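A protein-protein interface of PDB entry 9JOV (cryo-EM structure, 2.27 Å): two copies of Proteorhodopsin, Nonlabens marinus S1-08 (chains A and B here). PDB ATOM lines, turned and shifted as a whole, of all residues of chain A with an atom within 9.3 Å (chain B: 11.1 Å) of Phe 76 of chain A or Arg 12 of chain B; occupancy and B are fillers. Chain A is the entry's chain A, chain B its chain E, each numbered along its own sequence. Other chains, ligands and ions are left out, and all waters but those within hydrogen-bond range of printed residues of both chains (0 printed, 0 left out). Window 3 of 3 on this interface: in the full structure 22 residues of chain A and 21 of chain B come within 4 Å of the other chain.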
ATOM      1  N   VAL A  11      14.484 -31.836   6.465  1.00  0.00           N
ATOM      2  CA  VAL A  11      13.362 -31.132   7.172  1.00  0.00           C
ATOM      3  C   VAL A  11      12.092 -31.225   6.317  1.00  0.00           C
ATOM      4  O   VAL A  11      11.367 -30.249   6.110  1.00  0.00           O
ATOM      5  CB  VAL A  11      13.713 -29.668   7.505  1.00  0.00           C
ATOM      6  CG1 VAL A  11      12.626 -28.993   8.329  1.00  0.00           C
ATOM      7  CG2 VAL A  11      15.047 -29.547   8.238  1.00  0.00           C
ATOM      8  N   ASP A  17       2.607 -35.631  11.449  1.00  0.00           N
ATOM      9  CA  ASP A  17       3.136 -34.738  12.473  1.00  0.00           C
ATOM     10  C   ASP A  17       2.095 -33.665  12.807  1.00  0.00           C
ATOM     11  O   ASP A  17       2.164 -32.521  12.337  1.00  0.00           O
ATOM     12  CB  ASP A  17       4.469 -34.173  12.029  1.00  0.00           C
ATOM     13  CG  ASP A  17       5.144 -33.185  12.965  1.00  0.00           C
ATOM     14  OD1 ASP A  17       4.759 -33.179  14.135  1.00  0.00           O
ATOM     15  OD2 ASP A  17       6.072 -32.453  12.512  1.00  0.00           O
ATOM     16  N   TYR A  68       9.386 -18.833  16.156  1.00  0.00           N
ATOM     17  CA  TYR A  68      10.627 -19.461  16.591  1.00  0.00           C
ATOM     18  C   TYR A  68      10.326 -20.920  16.994  1.00  0.00           C
ATOM     19  O   TYR A  68      11.006 -21.852  16.590  1.00  0.00           O
ATOM     20  CB  TYR A  68      11.229 -18.655  17.754  1.00  0.00           C
ATOM     21  CG  TYR A  68      12.645 -19.079  18.071  1.00  0.00           C
ATOM     22  CD1 TYR A  68      12.900 -20.249  18.787  1.00  0.00           C
ATOM     23  CD2 TYR A  68      13.734 -18.345  17.607  1.00  0.00           C
ATOM     24  CE1 TYR A  68      14.193 -20.693  19.010  1.00  0.00           C
ATOM     25  CE2 TYR A  68      15.031 -18.777  17.820  1.00  0.00           C
ATOM     26  CZ  TYR A  68      15.259 -19.961  18.513  1.00  0.00           C
ATOM     27  OH  TYR A  68      16.529 -20.393  18.768  1.00  0.00           O
ATOM     28  N   MET A  69       9.311 -21.163  17.803  1.00  0.00           N
ATOM     29  CA  MET A  69       9.057 -22.530  18.205  1.00  0.00           C
ATOM     30  C   MET A  69       8.742 -23.459  17.023  1.00  0.00           C
ATOM     31  O   MET A  69       9.170 -24.624  17.015  1.00  0.00           O
ATOM     32  CB  MET A  69       7.925 -22.599  19.228  1.00  0.00           C
ATOM     33  CG  MET A  69       8.296 -21.920  20.550  1.00  0.00           C
ATOM     34  SD  MET A  69       7.072 -22.271  21.829  1.00  0.00           S
ATOM     35  CE  MET A  69       5.637 -21.321  21.294  1.00  0.00           C
ATOM     36  N   ARG A  70       7.994 -22.973  16.037  1.00  0.00           N
ATOM     37  CA  ARG A  70       7.686 -23.748  14.824  1.00  0.00           C
ATOM     38  C   ARG A  70       8.943 -24.195  14.105  1.00  0.00           C
ATOM     39  O   ARG A  70       9.050 -25.347  13.705  1.00  0.00           O
ATOM     40  CB  ARG A  70       6.954 -22.860  13.819  1.00  0.00           C
ATOM     41  CG  ARG A  70       6.581 -23.554  12.532  1.00  0.00           C
ATOM     42  CD  ARG A  70       6.053 -22.541  11.578  1.00  0.00           C
ATOM     43  NE  ARG A  70       7.134 -21.764  10.974  1.00  0.00           N
ATOM     44  CZ  ARG A  70       6.999 -20.739  10.161  1.00  0.00           C
ATOM     45  NH1 ARG A  70       5.839 -20.147   9.969  1.00  0.00           N
ATOM     46  NH2 ARG A  70       8.074 -20.286   9.567  1.00  0.00           N
ATOM     47  N   ASP A  71       9.909 -23.267  13.970  1.00  0.00           N
ATOM     48  CA  ASP A  71      11.138 -23.612  13.299  1.00  0.00           C
ATOM     49  C   ASP A  71      11.942 -24.594  14.137  1.00  0.00           C
ATOM     50  O   ASP A  71      12.453 -25.578  13.634  1.00  0.00           O
ATOM     51  CB  ASP A  71      11.902 -22.376  12.877  1.00  0.00           C
ATOM     52  CG  ASP A  71      11.268 -21.529  11.787  1.00  0.00           C
ATOM     53  OD1 ASP A  71      10.353 -22.032  11.103  1.00  0.00           O
ATOM     54  OD2 ASP A  71      11.707 -20.370  11.610  1.00  0.00           O
ATOM     55  N   TYR A  72      11.983 -24.376  15.442  1.00  0.00           N
ATOM     56  CA  TYR A  72      12.751 -25.262  16.283  1.00  0.00           C
ATOM     57  C   TYR A  72      12.187 -26.678  16.235  1.00  0.00           C
ATOM     58  O   TYR A  72      12.946 -27.640  16.215  1.00  0.00           O
ATOM     59  CB  TYR A  72      12.787 -24.678  17.680  1.00  0.00           C
ATOM     60  CG  TYR A  72      13.701 -25.449  18.619  1.00  0.00           C
ATOM     61  CD1 TYR A  72      13.211 -26.539  19.333  1.00  0.00           C
ATOM     62  CD2 TYR A  72      15.005 -25.036  18.863  1.00  0.00           C
ATOM     63  CE1 TYR A  72      13.996 -27.208  20.256  1.00  0.00           C
ATOM     64  CE2 TYR A  72      15.798 -25.696  19.791  1.00  0.00           C
ATOM     65  CZ  TYR A  72      15.297 -26.789  20.482  1.00  0.00           C
ATOM     66  OH  TYR A  72      16.042 -27.496  21.381  1.00  0.00           O
ATOM     67  N   TRP A  73      10.860 -26.815  16.216  1.00  0.00           N
ATOM     68  CA  TRP A  73      10.265 -28.141  16.078  1.00  0.00           C
ATOM     69  C   TRP A  73      10.598 -28.782  14.743  1.00  0.00           C
ATOM     70  O   TRP A  73      10.845 -29.990  14.699  1.00  0.00           O
ATOM     71  CB  TRP A  73       8.759 -28.058  16.202  1.00  0.00           C
ATOM     72  CG  TRP A  73       8.100 -29.382  15.995  1.00  0.00           C
ATOM     73  CD1 TRP A  73       7.551 -29.895  14.847  1.00  0.00           C
ATOM     74  CD2 TRP A  73       7.912 -30.363  17.019  1.00  0.00           C
ATOM     75  NE1 TRP A  73       7.039 -31.139  15.086  1.00  0.00           N
ATOM     76  CE2 TRP A  73       7.260 -31.458  16.400  1.00  0.00           C
ATOM     77  CE3 TRP A  73       8.227 -30.416  18.378  1.00  0.00           C
ATOM     78  CZ2 TRP A  73       6.920 -32.599  17.116  1.00  0.00           C
ATOM     79  CZ3 TRP A  73       7.869 -31.541  19.088  1.00  0.00           C
ATOM     80  CH2 TRP A  73       7.209 -32.610  18.464  1.00  0.00           C
ATOM     81  N   SER A  74      10.584 -27.995  13.656  1.00  0.00           N
ATOM     82  CA  SER A  74      11.027 -28.490  12.352  1.00  0.00           C
ATOM     83  C   SER A  74      12.446 -29.061  12.406  1.00  0.00           C
ATOM     84  O   SER A  74      12.699 -30.127  11.874  1.00  0.00           O
ATOM     85  CB  SER A  74      10.938 -27.433  11.322  1.00  0.00           C
ATOM     86  OG  SER A  74       9.578 -27.109  11.075  1.00  0.00           O
ATOM     87  N   GLY A  75      13.351 -28.388  13.115  1.00  0.00           N
ATOM     88  CA  GLY A  75      14.725 -28.845  13.250  1.00  0.00           C
ATOM     89  C   GLY A  75      14.867 -30.095  14.112  1.00  0.00           C
ATOM     90  O   GLY A  75      15.339 -31.118  13.631  1.00  0.00           O
ATOM     91  N   PHE A  76      14.437 -30.022  15.373  1.00  0.00           N
ATOM     92  CA  PHE A  76      14.802 -31.005  16.378  1.00  0.00           C
ATOM     93  C   PHE A  76      13.665 -31.942  16.786  1.00  0.00           C
ATOM     94  O   PHE A  76      13.910 -32.912  17.499  1.00  0.00           O
ATOM     95  CB  PHE A  76      15.229 -30.294  17.661  1.00  0.00           C
ATOM     96  CG  PHE A  76      16.432 -29.396  17.471  1.00  0.00           C
ATOM     97  CD1 PHE A  76      17.711 -29.926  17.515  1.00  0.00           C
ATOM     98  CD2 PHE A  76      16.281 -28.031  17.290  1.00  0.00           C
ATOM     99  CE1 PHE A  76      18.814 -29.111  17.345  1.00  0.00           C
ATOM    100  CE2 PHE A  76      17.388 -27.221  17.128  1.00  0.00           C
ATOM    101  CZ  PHE A  76      18.649 -27.766  17.144  1.00  0.00           C
ATOM    102  N   ALA A  77      12.432 -31.638  16.406  1.00  0.00           N
ATOM    103  CA  ALA A  77      11.292 -32.419  16.864  1.00  0.00           C
ATOM    104  C   ALA A  77      11.196 -32.460  18.387  1.00  0.00           C
ATOM    105  O   ALA A  77      10.750 -33.453  18.960  1.00  0.00           O
ATOM    106  CB  ALA A  77      11.357 -33.806  16.289  1.00  0.00           C
ATOM    107  N   GLU A  78      11.554 -31.349  19.035  1.00  0.00           N
ATOM    108  CA  GLU A  78      11.357 -31.171  20.465  1.00  0.00           C
ATOM    109  C   GLU A  78      10.746 -29.798  20.748  1.00  0.00           C
ATOM    110  O   GLU A  78      10.990 -28.809  20.066  1.00  0.00           O
ATOM    111  CB  GLU A  78      12.685 -31.277  21.204  1.00  0.00           C
ATOM    112  CG  GLU A  78      13.353 -32.644  21.101  1.00  0.00           C
ATOM    113  CD  GLU A  78      14.823 -32.613  21.504  1.00  0.00           C
ATOM    114  OE1 GLU A  78      15.366 -31.500  21.718  1.00  0.00           O
ATOM    115  OE2 GLU A  78      15.431 -33.702  21.615  1.00  0.00           O
ATOM    116  N   SER A  79       9.908 -29.738  21.774  1.00  0.00           N
ATOM    117  CA  SER A  79       9.417 -28.465  22.243  1.00  0.00           C
ATOM    118  C   SER A  79       9.499 -28.458  23.764  1.00  0.00           C
ATOM    119  O   SER A  79       8.554 -28.849  24.449  1.00  0.00           O
ATOM    120  CB  SER A  79       8.041 -28.191  21.756  1.00  0.00           C
ATOM    121  OG  SER A  79       7.704 -26.818  21.955  1.00  0.00           O
ATOM    122  N   PRO A  80      10.639 -28.013  24.336  1.00  0.00           N
ATOM    123  CA  PRO A  80      10.769 -27.921  25.784  1.00  0.00           C
ATOM    124  C   PRO A  80       9.790 -26.926  26.419  1.00  0.00           C
ATOM    125  O   PRO A  80       9.649 -25.787  25.987  1.00  0.00           O
ATOM    126  CB  PRO A  80      12.227 -27.542  25.962  1.00  0.00           C
ATOM    127  CG  PRO A  80      12.683 -26.941  24.620  1.00  0.00           C
ATOM    128  CD  PRO A  80      11.813 -27.545  23.584  1.00  0.00           C
ATOM    129  N   PHE A  82       9.762 -25.301  29.127  1.00  0.00           N
ATOM    130  CA  PHE A  82      10.282 -24.092  29.738  1.00  0.00           C
ATOM    131  C   PHE A  82      10.366 -22.985  28.688  1.00  0.00           C
ATOM    132  O   PHE A  82      10.172 -21.826  29.010  1.00  0.00           O
ATOM    133  CB  PHE A  82      11.650 -24.245  30.399  1.00  0.00           C
ATOM    134  CG  PHE A  82      12.768 -24.327  29.398  1.00  0.00           C
ATOM    135  CD1 PHE A  82      13.287 -23.163  28.842  1.00  0.00           C
ATOM    136  CD2 PHE A  82      13.308 -25.548  29.032  1.00  0.00           C
ATOM    137  CE1 PHE A  82      14.311 -23.231  27.914  1.00  0.00           C
ATOM    138  CE2 PHE A  82      14.310 -25.604  28.091  1.00  0.00           C
ATOM    139  CZ  PHE A  82      14.787 -24.450  27.511  1.00  0.00           C
ATOM    140  N   PHE A  83      10.558 -23.345  27.423  1.00  0.00           N
ATOM    141  CA  PHE A  83      10.711 -22.336  26.409  1.00  0.00           C
ATOM    142  C   PHE A  83       9.379 -21.637  26.123  1.00  0.00           C
ATOM    143  O   PHE A  83       9.370 -20.523  25.603  1.00  0.00           O
ATOM    144  CB  PHE A  83      11.274 -22.981  25.157  1.00  0.00           C
ATOM    145  CG  PHE A  83      11.839 -21.986  24.165  1.00  0.00           C
ATOM    146  CD1 PHE A  83      12.857 -21.117  24.536  1.00  0.00           C
ATOM    147  CD2 PHE A  83      11.389 -21.959  22.859  1.00  0.00           C
ATOM    148  CE1 PHE A  83      13.423 -20.245  23.606  1.00  0.00           C
ATOM    149  CE2 PHE A  83      11.937 -21.074  21.946  1.00  0.00           C
ATOM    150  CZ  PHE A  83      12.954 -20.219  22.317  1.00  0.00           C
ATOM    151  N   VAL B  11      22.688 -24.993  18.799  1.00  0.00           N
ATOM    152  CA  VAL B  11      21.454 -24.166  18.968  1.00  0.00           C
ATOM    153  C   VAL B  11      20.321 -24.984  19.590  1.00  0.00           C
ATOM    154  O   VAL B  11      19.203 -24.504  19.567  1.00  0.00           O
ATOM    155  CB  VAL B  11      20.991 -23.507  17.648  1.00  0.00           C
ATOM    156  CG1 VAL B  11      21.861 -22.315  17.273  1.00  0.00           C
ATOM    157  CG2 VAL B  11      20.908 -24.508  16.500  1.00  0.00           C
ATOM    158  N   ARG B  12      20.589 -26.152  20.200  1.00  0.00           N
ATOM    159  CA  ARG B  12      19.613 -26.774  21.083  1.00  0.00           C
ATOM    160  C   ARG B  12      19.531 -25.969  22.381  1.00  0.00           C
ATOM    161  O   ARG B  12      20.549 -25.509  22.871  1.00  0.00           O
ATOM    162  CB  ARG B  12      19.963 -28.239  21.352  1.00  0.00           C
ATOM    163  CG  ARG B  12      18.727 -29.077  21.640  1.00  0.00           C
ATOM    164  CD  ARG B  12      19.016 -30.537  21.905  1.00  0.00           C
ATOM    165  NE  ARG B  12      19.634 -31.170  20.737  1.00  0.00           N
ATOM    166  CZ  ARG B  12      19.071 -32.062  19.925  1.00  0.00           C
ATOM    167  NH1 ARG B  12      17.815 -32.438  20.094  1.00  0.00           N
ATOM    168  NH2 ARG B  12      19.774 -32.565  18.926  1.00  0.00           N
ATOM    169  N   LEU B  13      18.314 -25.777  22.898  1.00  0.00           N
ATOM    170  CA  LEU B  13      18.083 -24.928  24.057  1.00  0.00           C
ATOM    171  C   LEU B  13      18.291 -25.762  25.319  1.00  0.00           C
ATOM    172  O   LEU B  13      17.880 -26.928  25.356  1.00  0.00           O
ATOM    173  CB  LEU B  13      16.661 -24.385  24.085  1.00  0.00           C
ATOM    174  CG  LEU B  13      16.134 -23.679  22.838  1.00  0.00           C
ATOM    175  CD1 LEU B  13      14.638 -23.943  22.672  1.00  0.00           C
ATOM    176  CD2 LEU B  13      16.477 -22.210  22.961  1.00  0.00           C
ATOM    177  N   ALA B  14      18.846 -25.143  26.368  1.00  0.00           N
ATOM    178  CA  ALA B  14      18.989 -25.806  27.653  1.00  0.00           C
ATOM    179  C   ALA B  14      18.194 -25.072  28.723  1.00  0.00           C
ATOM    180  O   ALA B  14      18.228 -23.847  28.780  1.00  0.00           O
ATOM    181  CB  ALA B  14      20.444 -25.887  28.041  1.00  0.00           C
ATOM    182  N   ALA B  15      17.529 -25.852  29.582  1.00  0.00           N
ATOM    183  CA  ALA B  15      16.702 -25.332  30.657  1.00  0.00           C
ATOM    184  C   ALA B  15      17.504 -24.523  31.671  1.00  0.00           C
ATOM    185  O   ALA B  15      16.967 -23.571  32.242  1.00  0.00           O
ATOM    186  CB  ALA B  15      15.999 -26.471  31.337  1.00  0.00           C
ATOM    187  N   ASP B  16      18.789 -24.845  31.854  1.00  0.00           N
ATOM    188  CA  ASP B  16      19.619 -24.137  32.829  1.00  0.00           C
ATOM    189  C   ASP B  16      20.291 -22.900  32.228  1.00  0.00           C
ATOM    190  O   ASP B  16      21.044 -22.231  32.930  1.00  0.00           O
ATOM    191  CB  ASP B  16      20.725 -25.024  33.381  1.00  0.00           C
ATOM    192  CG  ASP B  16      21.574 -25.736  32.334  1.00  0.00           C
ATOM    193  OD1 ASP B  16      22.013 -25.101  31.328  1.00  0.00           O
ATOM    194  OD2 ASP B  16      21.751 -26.946  32.507  1.00  0.00           O
ATOM    195  N   ASP B  17      20.079 -22.604  30.934  1.00  0.00           N
ATOM    196  CA  ASP B  17      20.682 -21.417  30.352  1.00  0.00           C
ATOM    197  C   ASP B  17      19.817 -20.185  30.639  1.00  0.00           C
ATOM    198  O   ASP B  17      19.067 -19.725  29.775  1.00  0.00           O
ATOM    199  CB  ASP B  17      20.938 -21.604  28.875  1.00  0.00           C
ATOM    200  CG  ASP B  17      21.638 -20.456  28.155  1.00  0.00           C
ATOM    201  OD1 ASP B  17      22.158 -19.553  28.831  1.00  0.00           O
ATOM    202  OD2 ASP B  17      21.623 -20.468  26.899  1.00  0.00           O
ATOM    203  N   TYR B  18      20.002 -19.600  31.826  1.00  0.00           N
ATOM    204  CA  TYR B  18      19.223 -18.455  32.250  1.00  0.00           C
ATOM    205  C   TYR B  18      19.633 -17.190  31.483  1.00  0.00           C
ATOM    206  O   TYR B  18      18.836 -16.252  31.365  1.00  0.00           O
ATOM    207  CB  TYR B  18      19.425 -18.250  33.755  1.00  0.00           C
ATOM    208  CG  TYR B  18      19.288 -19.555  34.520  1.00  0.00           C
ATOM    209  CD1 TYR B  18      18.194 -20.390  34.313  1.00  0.00           C
ATOM    210  CD2 TYR B  18      20.299 -20.004  35.364  1.00  0.00           C
ATOM    211  CE1 TYR B  18      18.070 -21.598  34.984  1.00  0.00           C
ATOM    212  CE2 TYR B  18      20.182 -21.202  36.045  1.00  0.00           C
ATOM    213  CZ  TYR B  18      19.070 -22.006  35.850  1.00  0.00           C
ATOM    214  OH  TYR B  18      18.977 -23.204  36.504  1.00  0.00           O
ATOM    215  N   GLY B  20      20.405 -17.287  28.347  1.00  0.00           N
ATOM    216  CA  GLY B  20      19.671 -17.498  27.117  1.00  0.00           C
ATOM    217  C   GLY B  20      18.222 -17.060  27.269  1.00  0.00           C
ATOM    218  O   GLY B  20      17.688 -16.354  26.425  1.00  0.00           O
ATOM    219  N   PHE B  21      17.604 -17.465  28.367  1.00  0.00           N
ATOM    220  CA  PHE B  21      16.197 -17.200  28.574  1.00  0.00           C
ATOM    221  C   PHE B  21      15.937 -15.693  28.613  1.00  0.00           C
ATOM    222  O   PHE B  21      14.992 -15.196  28.012  1.00  0.00           O
ATOM    223  CB  PHE B  21      15.830 -17.934  29.876  1.00  0.00           C
ATOM    224  CG  PHE B  21      14.339 -17.829  30.149  1.00  0.00           C
ATOM    225  CD1 PHE B  21      13.457 -18.683  29.505  1.00  0.00           C
ATOM    226  CD2 PHE B  21      13.824 -16.857  31.016  1.00  0.00           C
ATOM    227  CE1 PHE B  21      12.080 -18.576  29.719  1.00  0.00           C
ATOM    228  CE2 PHE B  21      12.458 -16.750  31.227  1.00  0.00           C
ATOM    229  CZ  PHE B  21      11.583 -17.598  30.565  1.00  0.00           C
ATOM    230  N   PHE B  24      15.877 -13.962  25.276  1.00  0.00           N
ATOM    231  CA  PHE B  24      14.619 -14.151  24.554  1.00  0.00           C
ATOM    232  C   PHE B  24      13.505 -13.277  25.122  1.00  0.00           C
ATOM    233  O   PHE B  24      12.757 -12.649  24.382  1.00  0.00           O
ATOM    234  CB  PHE B  24      14.134 -15.583  24.561  1.00  0.00           C
ATOM    235  CG  PHE B  24      14.740 -16.453  23.466  1.00  0.00           C
ATOM    236  CD1 PHE B  24      15.965 -17.081  23.656  1.00  0.00           C
ATOM    237  CD2 PHE B  24      14.113 -16.580  22.222  1.00  0.00           C
ATOM    238  CE1 PHE B  24      16.549 -17.845  22.650  1.00  0.00           C
ATOM    239  CE2 PHE B  24      14.667 -17.398  21.238  1.00  0.00           C
ATOM    240  CZ  PHE B  24      15.881 -18.041  21.465  1.00  0.00           C
ATOM    241  N   ARG B  70      20.838 -12.016  21.112  1.00  0.00           N
ATOM    242  CA  ARG B  70      20.214 -13.308  21.404  1.00  0.00           C
ATOM    243  C   ARG B  70      20.730 -14.395  20.476  1.00  0.00           C
ATOM    244  O   ARG B  70      21.048 -15.490  20.934  1.00  0.00           O
ATOM    245  CB  ARG B  70      18.711 -13.262  21.121  1.00  0.00           C
ATOM    246  CG  ARG B  70      17.993 -14.571  21.391  1.00  0.00           C
ATOM    247  CD  ARG B  70      16.584 -14.430  20.874  1.00  0.00           C
ATOM    248  NE  ARG B  70      16.524 -14.567  19.431  1.00  0.00           N
ATOM    249  CZ  ARG B  70      15.450 -14.389  18.675  1.00  0.00           C
ATOM    250  NH1 ARG B  70      14.330 -13.856  19.125  1.00  0.00           N
ATOM    251  NH2 ARG B  70      15.528 -14.735  17.404  1.00  0.00           N
ATOM    252  N   ASP B  71      20.834 -14.081  19.174  1.00  0.00           N
ATOM    253  CA  ASP B  71      21.312 -15.083  18.233  1.00  0.00           C
ATOM    254  C   ASP B  71      22.781 -15.353  18.482  1.00  0.00           C
ATOM    255  O   ASP B  71      23.203 -16.496  18.509  1.00  0.00           O
ATOM    256  CB  ASP B  71      20.991 -14.709  16.797  1.00  0.00           C
ATOM    257  CG  ASP B  71      19.516 -14.741  16.421  1.00  0.00           C
ATOM    258  OD1 ASP B  71      18.725 -15.370  17.174  1.00  0.00           O
ATOM    259  OD2 ASP B  71      19.175 -14.144  15.366  1.00  0.00           O
ATOM    260  N   TRP B  73      24.430 -15.178  21.250  1.00  0.00           N
ATOM    261  CA  TRP B  73      24.558 -16.041  22.417  1.00  0.00           C
ATOM    262  C   TRP B  73      24.188 -17.489  22.113  1.00  0.00           C
ATOM    263  O   TRP B  73      24.845 -18.393  22.609  1.00  0.00           O
ATOM    264  CB  TRP B  73      23.665 -15.547  23.537  1.00  0.00           C
ATOM    265  CG  TRP B  73      23.728 -16.444  24.725  1.00  0.00           C
ATOM    266  CD1 TRP B  73      22.876 -17.454  25.079  1.00  0.00           C
ATOM    267  CD2 TRP B  73      24.716 -16.353  25.760  1.00  0.00           C
ATOM    268  NE1 TRP B  73      23.277 -18.022  26.267  1.00  0.00           N
ATOM    269  CE2 TRP B  73      24.405 -17.368  26.702  1.00  0.00           C
ATOM    270  CE3 TRP B  73      25.801 -15.500  25.981  1.00  0.00           C
ATOM    271  CZ2 TRP B  73      25.157 -17.539  27.852  1.00  0.00           C
ATOM    272  CZ3 TRP B  73      26.539 -15.668  27.133  1.00  0.00           C
ATOM    273  CH2 TRP B  73      26.199 -16.657  28.065  1.00  0.00           C
ATOM    274  N   SER B  74      23.118 -17.703  21.332  1.00  0.00           N
ATOM    275  CA  SER B  74      22.773 -19.038  20.866  1.00  0.00           C
ATOM    276  C   SER B  74      23.950 -19.717  20.141  1.00  0.00           C
ATOM    277  O   SER B  74      24.247 -20.876  20.392  1.00  0.00           O
ATOM    278  CB  SER B  74      21.591 -19.002  19.989  1.00  0.00           C
ATOM    279  OG  SER B  74      20.436 -18.633  20.725  1.00  0.00           O
ATOM    280  N   GLY B  75      24.669 -18.973  19.298  1.00  0.00           N
ATOM    281  CA  GLY B  75      25.819 -19.489  18.587  1.00  0.00           C
ATOM    282  C   GLY B  75      27.020 -19.789  19.486  1.00  0.00           C
ATOM    283  O   GLY B  75      27.455 -20.931  19.576  1.00  0.00           O
ATOM    284  N   PHE B  76      27.535 -18.768  20.162  1.00  0.00           N
ATOM    285  CA  PHE B  76      28.852 -18.820  20.773  1.00  0.00           C
ATOM    286  C   PHE B  76      28.826 -18.900  22.299  1.00  0.00           C
ATOM    287  O   PHE B  76      29.865 -19.134  22.910  1.00  0.00           O
ATOM    288  CB  PHE B  76      29.633 -17.550  20.449  1.00  0.00           C
ATOM    289  CG  PHE B  76      29.830 -17.327  18.965  1.00  0.00           C
ATOM    290  CD1 PHE B  76      30.849 -17.976  18.281  1.00  0.00           C
ATOM    291  CD2 PHE B  76      29.018 -16.441  18.274  1.00  0.00           C
ATOM    292  CE1 PHE B  76      31.024 -17.769  16.928  1.00  0.00           C
ATOM    293  CE2 PHE B  76      29.204 -16.234  16.920  1.00  0.00           C
ATOM    294  CZ  PHE B  76      30.200 -16.902  16.250  1.00  0.00           C
ATOM    295  N   ALA B  77      27.674 -18.673  22.927  1.00  0.00           N
ATOM    296  CA  ALA B  77      27.608 -18.630  24.379  1.00  0.00           C
ATOM    297  C   ALA B  77      28.553 -17.575  24.960  1.00  0.00           C
ATOM    298  O   ALA B  77      29.091 -17.743  26.051  1.00  0.00           O
ATOM    299  CB  ALA B  77      27.886 -19.988  24.948  1.00  0.00           C
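N of Leu 13 of chain B is in hydrogen-bond range of OH of Tyr 72 of chain A (3.2 Å).
The side-chain carboxylate (OE1) of Glu 78 of chain A is in salt-bridge range of the guanidinium group (NH1) of Arg 12 of chain B (3.1 Å).
No residue of chain B comes within 4 Å of Gly 75 of chain A.
Of the printed residues of chain B, Phe 76 of chain A touches Arg 12.
No residue of chain B comes within 4 Å of Ala 77 of chain A.
Glu 78 of chain A touches just one residue of chain B: Arg 12 (3.1 Å).
Printed residues of chain B within 4 Å of Phe 82 of chain A: Leu 13 (3.9 Å), Ala 14 (3.7 Å), Ala 15 (3.5 Å) and Phe 21 (3.8 Å).
Of the printed residues of chain B, Phe 83 of chain A touches Leu 13 (3.7 Å) and Phe 24 (3.5 Å).
Arg 12 of chain B touches just these residues of chain A: Tyr 72, Phe 76 and Glu 78.
Of the printed residues of chain A, Leu 13 of chain B touches Tyr 72 (3.2 Å), Phe 82 (3.9 Å) and Phe 83 (3.7 Å).
Among the printed residues, merely in contact across the chains: Tyr 68 of chain A with Phe 24 of chain B, Tyr 72 of chain A with Val 11 of chain B, Tyr 72 of chain A with Arg 12 of chain B, Phe 76 of chain A with Arg 12 of chain B, Phe 82 of chain A with Leu 13 of chain B, Phe 82 of chain A with Ala 14 of chain B, Phe 82 of chain A with Ala 15 of chain B, Phe 82 of chain A with Phe 21 of chain B, Phe 83 of chain A with Leu 13 of chain B and Phe 83 of chain A with Phe 24 of chain B.
Printed residues of chain A that touch a printed residue of chain B: Tyr 68, Tyr 72, Phe 76, Glu 78, Phe 82 and Phe 83.
Hydrophobic or aromatic side chains of chain B that line the printed part of chain A: Leu 13, Ala 15, Phe 21 and Phe 24.
Among the printed residues, 12 pairs touch across the chains.
9 positions are printed for both chains.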
